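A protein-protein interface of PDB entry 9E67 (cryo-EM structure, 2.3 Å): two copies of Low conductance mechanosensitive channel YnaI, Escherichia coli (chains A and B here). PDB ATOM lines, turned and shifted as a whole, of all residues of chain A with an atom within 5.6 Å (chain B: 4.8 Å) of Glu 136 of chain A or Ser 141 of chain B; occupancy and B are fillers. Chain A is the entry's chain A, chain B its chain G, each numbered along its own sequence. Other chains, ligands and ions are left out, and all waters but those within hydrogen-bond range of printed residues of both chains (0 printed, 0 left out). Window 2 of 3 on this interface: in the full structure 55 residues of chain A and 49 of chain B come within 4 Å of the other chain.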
ATOM      1  N   LEU A 132     -25.276  26.477  -1.756  1.00  0.00           N
ATOM      2  CA  LEU A 132     -24.473  26.262  -2.955  1.00  0.00           C
ATOM      3  C   LEU A 132     -23.218  27.130  -2.947  1.00  0.00           C
ATOM      4  O   LEU A 132     -22.161  26.702  -3.420  1.00  0.00           O
ATOM      5  CB  LEU A 132     -25.333  26.522  -4.199  1.00  0.00           C
ATOM      6  CG  LEU A 132     -24.801  26.537  -5.640  1.00  0.00           C
ATOM      7  CD1 LEU A 132     -23.973  27.775  -5.987  1.00  0.00           C
ATOM      8  CD2 LEU A 132     -23.999  25.272  -5.911  1.00  0.00           C
ATOM      9  N   LEU A 133     -23.315  28.350  -2.418  1.00  0.00           N
ATOM     10  CA  LEU A 133     -22.183  29.270  -2.479  1.00  0.00           C
ATOM     11  C   LEU A 133     -21.162  28.993  -1.378  1.00  0.00           C
ATOM     12  O   LEU A 133     -19.956  28.932  -1.638  1.00  0.00           O
ATOM     13  CB  LEU A 133     -22.678  30.716  -2.399  1.00  0.00           C
ATOM     14  CG  LEU A 133     -22.147  31.663  -3.477  1.00  0.00           C
ATOM     15  CD1 LEU A 133     -22.278  31.037  -4.856  1.00  0.00           C
ATOM     16  CD2 LEU A 133     -22.869  32.998  -3.423  1.00  0.00           C
ATOM     17  N   TYR A 134     -21.626  28.822  -0.140  1.00  0.00           N
ATOM     18  CA  TYR A 134     -20.748  28.654   1.011  1.00  0.00           C
ATOM     19  C   TYR A 134     -20.473  27.189   1.330  1.00  0.00           C
ATOM     20  O   TYR A 134     -19.948  26.885   2.406  1.00  0.00           O
ATOM     21  CB  TYR A 134     -21.339  29.349   2.237  1.00  0.00           C
ATOM     22  CG  TYR A 134     -20.962  30.807   2.369  1.00  0.00           C
ATOM     23  CD1 TYR A 134     -20.956  31.645   1.262  1.00  0.00           C
ATOM     24  CD2 TYR A 134     -20.628  31.347   3.602  1.00  0.00           C
ATOM     25  CE1 TYR A 134     -20.619  32.979   1.381  1.00  0.00           C
ATOM     26  CE2 TYR A 134     -20.287  32.679   3.729  1.00  0.00           C
ATOM     27  CZ  TYR A 134     -20.284  33.490   2.616  1.00  0.00           C
ATOM     28  OH  TYR A 134     -19.945  34.818   2.740  1.00  0.00           O
ATOM     29  N   GLY A 135     -20.814  26.278   0.425  1.00  0.00           N
ATOM     30  CA  GLY A 135     -20.673  24.862   0.697  1.00  0.00           C
ATOM     31  C   GLY A 135     -19.259  24.323   0.608  1.00  0.00           C
ATOM     32  O   GLY A 135     -19.024  23.302  -0.043  1.00  0.00           O
ATOM     33  N   GLU A 136     -18.304  24.997   1.245  1.00  0.00           N
ATOM     34  CA  GLU A 136     -16.947  24.481   1.356  1.00  0.00           C
ATOM     35  C   GLU A 136     -16.401  24.465   2.773  1.00  0.00           C
ATOM     36  O   GLU A 136     -15.725  23.501   3.141  1.00  0.00           O
ATOM     37  CB  GLU A 136     -15.987  25.296   0.477  1.00  0.00           C
ATOM     38  CG  GLU A 136     -16.095  24.997  -1.001  1.00  0.00           C
ATOM     39  CD  GLU A 136     -14.750  24.721  -1.636  1.00  0.00           C
ATOM     40  OE1 GLU A 136     -14.717  24.349  -2.827  1.00  0.00           O
ATOM     41  OE2 GLU A 136     -13.722  24.873  -0.943  1.00  0.00           O
ATOM     42  N   HIS A 137     -16.673  25.493   3.580  1.00  0.00           N
ATOM     43  CA  HIS A 137     -16.155  25.520   4.940  1.00  0.00           C
ATOM     44  C   HIS A 137     -16.770  24.431   5.805  1.00  0.00           C
ATOM     45  O   HIS A 137     -16.056  23.802   6.594  1.00  0.00           O
ATOM     46  CB  HIS A 137     -16.389  26.895   5.559  1.00  0.00           C
ATOM     47  CG  HIS A 137     -15.796  28.016   4.764  1.00  0.00           C
ATOM     48  ND1 HIS A 137     -14.440  28.146   4.559  1.00  0.00           N
ATOM     49  CD2 HIS A 137     -16.375  29.054   4.117  1.00  0.00           C
ATOM     50  CE1 HIS A 137     -14.209  29.218   3.822  1.00  0.00           C
ATOM     51  NE2 HIS A 137     -15.365  29.787   3.541  1.00  0.00           N
ATOM     52  N   PHE A 138     -18.073  24.197   5.672  1.00  0.00           N
ATOM     53  CA  PHE A 138     -18.682  22.988   6.207  1.00  0.00           C
ATOM     54  C   PHE A 138     -19.184  22.090   5.085  1.00  0.00           C
ATOM     55  O   PHE A 138     -19.898  21.117   5.362  1.00  0.00           O
ATOM     56  CB  PHE A 138     -19.831  23.327   7.166  1.00  0.00           C
ATOM     57  CG  PHE A 138     -20.726  24.429   6.674  1.00  0.00           C
ATOM     58  CD1 PHE A 138     -21.696  24.175   5.718  1.00  0.00           C
ATOM     59  CD2 PHE A 138     -20.602  25.716   7.171  1.00  0.00           C
ATOM     60  CE1 PHE A 138     -22.524  25.186   5.265  1.00  0.00           C
ATOM     61  CE2 PHE A 138     -21.425  26.729   6.722  1.00  0.00           C
ATOM     62  CZ  PHE A 138     -22.386  26.464   5.768  1.00  0.00           C
ATOM     63  N   GLY A 139     -18.821  22.374   3.837  1.00  0.00           N
ATOM     64  CA  GLY A 139     -19.344  21.656   2.692  1.00  0.00           C
ATOM     65  C   GLY A 139     -18.581  20.387   2.392  1.00  0.00           C
ATOM     66  O   GLY A 139     -17.720  19.949   3.163  1.00  0.00           O
ATOM     67  N   MET A 140     -18.901  19.786   1.253  1.00  0.00           N
ATOM     68  CA  MET A 140     -18.441  18.441   0.926  1.00  0.00           C
ATOM     69  C   MET A 140     -18.080  18.397  -0.556  1.00  0.00           C
ATOM     70  O   MET A 140     -17.819  19.429  -1.185  1.00  0.00           O
ATOM     71  CB  MET A 140     -19.489  17.381   1.295  1.00  0.00           C
ATOM     72  CG  MET A 140     -20.368  17.723   2.479  1.00  0.00           C
ATOM     73  SD  MET A 140     -21.577  16.429   2.743  1.00  0.00           S
ATOM     74  CE  MET A 140     -20.465  15.024   2.748  1.00  0.00           C
ATOM     75  N   LEU A 142     -16.771  18.337  -4.134  1.00  0.00           N
ATOM     76  CA  LEU A 142     -16.903  19.285  -5.232  1.00  0.00           C
ATOM     77  C   LEU A 142     -17.657  18.692  -6.411  1.00  0.00           C
ATOM     78  O   LEU A 142     -18.441  19.402  -7.046  1.00  0.00           O
ATOM     79  CB  LEU A 142     -15.525  19.769  -5.679  1.00  0.00           C
ATOM     80  CG  LEU A 142     -14.801  20.720  -4.722  1.00  0.00           C
ATOM     81  CD1 LEU A 142     -15.793  21.664  -4.061  1.00  0.00           C
ATOM     82  CD2 LEU A 142     -13.991  19.958  -3.680  1.00  0.00           C
ATOM     83  N   LEU A 145     -21.482  18.715  -5.403  1.00  0.00           N
ATOM     84  CA  LEU A 145     -22.053  20.057  -5.441  1.00  0.00           C
ATOM     85  C   LEU A 145     -22.132  20.584  -6.867  1.00  0.00           C
ATOM     86  O   LEU A 145     -23.132  21.204  -7.252  1.00  0.00           O
ATOM     87  CB  LEU A 145     -21.236  21.003  -4.561  1.00  0.00           C
ATOM     88  CG  LEU A 145     -21.879  21.385  -3.225  1.00  0.00           C
ATOM     89  CD1 LEU A 145     -22.440  20.163  -2.516  1.00  0.00           C
ATOM     90  CD2 LEU A 145     -20.878  22.104  -2.344  1.00  0.00           C
ATOM     91  N   GLY B 139     -13.620  36.197  -2.637  1.00  0.00           N
ATOM     92  CA  GLY B 139     -14.755  35.385  -3.030  1.00  0.00           C
ATOM     93  C   GLY B 139     -14.892  34.109  -2.234  1.00  0.00           C
ATOM     94  O   GLY B 139     -14.420  33.996  -1.096  1.00  0.00           O
ATOM     95  N   MET B 140     -15.539  33.125  -2.847  1.00  0.00           N
ATOM     96  CA  MET B 140     -15.948  31.907  -2.158  1.00  0.00           C
ATOM     97  C   MET B 140     -15.723  30.726  -3.095  1.00  0.00           C
ATOM     98  O   MET B 140     -14.970  30.819  -4.074  1.00  0.00           O
ATOM     99  CB  MET B 140     -17.404  32.025  -1.680  1.00  0.00           C
ATOM    100  CG  MET B 140     -17.603  32.870  -0.425  1.00  0.00           C
ATOM    101  SD  MET B 140     -17.284  32.009   1.133  1.00  0.00           S
ATOM    102  CE  MET B 140     -15.512  32.203   1.319  1.00  0.00           C
ATOM    103  N   SER B 141     -16.363  29.604  -2.770  1.00  0.00           N
ATOM    104  CA  SER B 141     -16.204  28.316  -3.435  1.00  0.00           C
ATOM    105  C   SER B 141     -16.069  28.435  -4.946  1.00  0.00           C
ATOM    106  O   SER B 141     -16.860  29.120  -5.603  1.00  0.00           O
ATOM    107  CB  SER B 141     -17.406  27.429  -3.096  1.00  0.00           C
ATOM    108  OG  SER B 141     -17.381  26.228  -3.849  1.00  0.00           O
ATOM    109  N   LEU B 142     -15.058  27.760  -5.492  1.00  0.00           N
ATOM    110  CA  LEU B 142     -14.914  27.643  -6.937  1.00  0.00           C
ATOM    111  C   LEU B 142     -16.106  26.942  -7.569  1.00  0.00           C
ATOM    112  O   LEU B 142     -16.628  27.418  -8.584  1.00  0.00           O
ATOM    113  CB  LEU B 142     -13.632  26.875  -7.263  1.00  0.00           C
ATOM    114  CG  LEU B 142     -12.400  27.654  -7.724  1.00  0.00           C
ATOM    115  CD1 LEU B 142     -12.556  28.112  -9.159  1.00  0.00           C
ATOM    116  CD2 LEU B 142     -12.142  28.836  -6.802  1.00  0.00           C
ATOM    117  N   SER B 143     -16.552  25.832  -6.978  1.00  0.00           N
ATOM    118  CA  SER B 143     -17.721  25.123  -7.486  1.00  0.00           C
ATOM    119  C   SER B 143     -18.969  25.995  -7.425  1.00  0.00           C
ATOM    120  O   SER B 143     -19.763  26.015  -8.370  1.00  0.00           O
ATOM    121  CB  SER B 143     -17.931  23.833  -6.693  1.00  0.00           C
ATOM    122  OG  SER B 143     -19.158  23.216  -7.036  1.00  0.00           O
ATOM    123  N   GLY B 144     -19.159  26.716  -6.318  1.00  0.00           N
ATOM    124  CA  GLY B 144     -20.340  27.551  -6.189  1.00  0.00           C
ATOM    125  C   GLY B 144     -20.393  28.659  -7.223  1.00  0.00           C
ATOM    126  O   GLY B 144     -21.432  28.882  -7.852  1.00  0.00           O
ATOM    127  N   LEU B 145     -19.278  29.366  -7.414  1.00  0.00           N
ATOM    128  CA  LEU B 145     -19.241  30.425  -8.417  1.00  0.00           C
ATOM    129  C   LEU B 145     -19.410  29.863  -9.822  1.00  0.00           C
ATOM    130  O   LEU B 145     -20.135  30.437 -10.643  1.00  0.00           O
ATOM    131  CB  LEU B 145     -17.940  31.215  -8.310  1.00  0.00           C
ATOM    132  CG  LEU B 145     -18.061  32.606  -7.687  1.00  0.00           C
ATOM    133  CD1 LEU B 145     -18.887  32.569  -6.409  1.00  0.00           C
ATOM    134  CD2 LEU B 145     -16.689  33.191  -7.428  1.00  0.00           C
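OG of Ser 141 of chain B lies close to OE1 of Glu 136 of chain A. A ring nitrogen (NE2) of His 137 of chain A sits close to the side-chain sulfur of Met 140 of chain B (3.8 Å).
The backbone NH of Ser 143 of chain B lies within hydrogen-bond range of the side-chain hydroxyl of Ser 141 of chain B (3.3 Å). N of Gly 144 of chain B lies within hydrogen-bond range of OG of Ser 141 of chain B (3.1 Å).
Among the printed residues, pairs that only touch across the chains: Leu 133 of chain A with Ser 141 of chain B (3.3 Å), Leu 132 of chain A with Gly 144 of chain B (3.3 Å), Tyr 134 of chain A with Met 140 of chain B (3.5 Å), Leu 133 of chain A with Gly 144 of chain B (3.8 Å), Leu 142 of chain A with Ser 143 of chain B (3.9 Å) and Leu 145 of chain A with Ser 143 of chain B (3.9 Å).
Glu 136 of chain A touches just one residue of chain B: Ser 141. Of the printed residues of chain A, Ser 141 of chain B touches Leu 133 (3.3 Å) and Glu 136 (3.4 Å). Of the printed residues of chain B, Leu 133 of chain A touches Ser 141 and Gly 144. Printed residues of chain B within 4 Å of Leu 132 of chain A: Gly 144. Printed residues of chain B within 4 Å of Leu 145 of chain A: Ser 143. The nearest printed residue of chain B that does not touch His 137 of chain A is Gly 139 of chain B (6.3 Å).
Hydrophobic or aromatic side chains of chain B that line the printed part of chain A: Met 140. Along chain B the printed residues that touch a printed residue of chain A span positions 140 to 144. Of the 11 printed residues of chain A, 7 touch a printed residue of chain B. Hydrophobic or aromatic side chains of chain A within 4 Å of the printed part of chain B: Leu 132, Leu 133, Tyr 134, His 137 and Leu 145. Along chain A the printed residues that touch a printed residue of chain B span positions 132 to 145. Among the printed residues, 8 pairs touch across the chains. Among the printed residues, no Asp or Glu carboxylate lies within 4 Å of a Lys or Arg side-chain nitrogen of the other chain.
Positions printed for both chains: 139, 140, 142 and 145. Of the 8 pairs that touch across the chains among the printed residues, none has its exchanged pair printed and touching as well.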
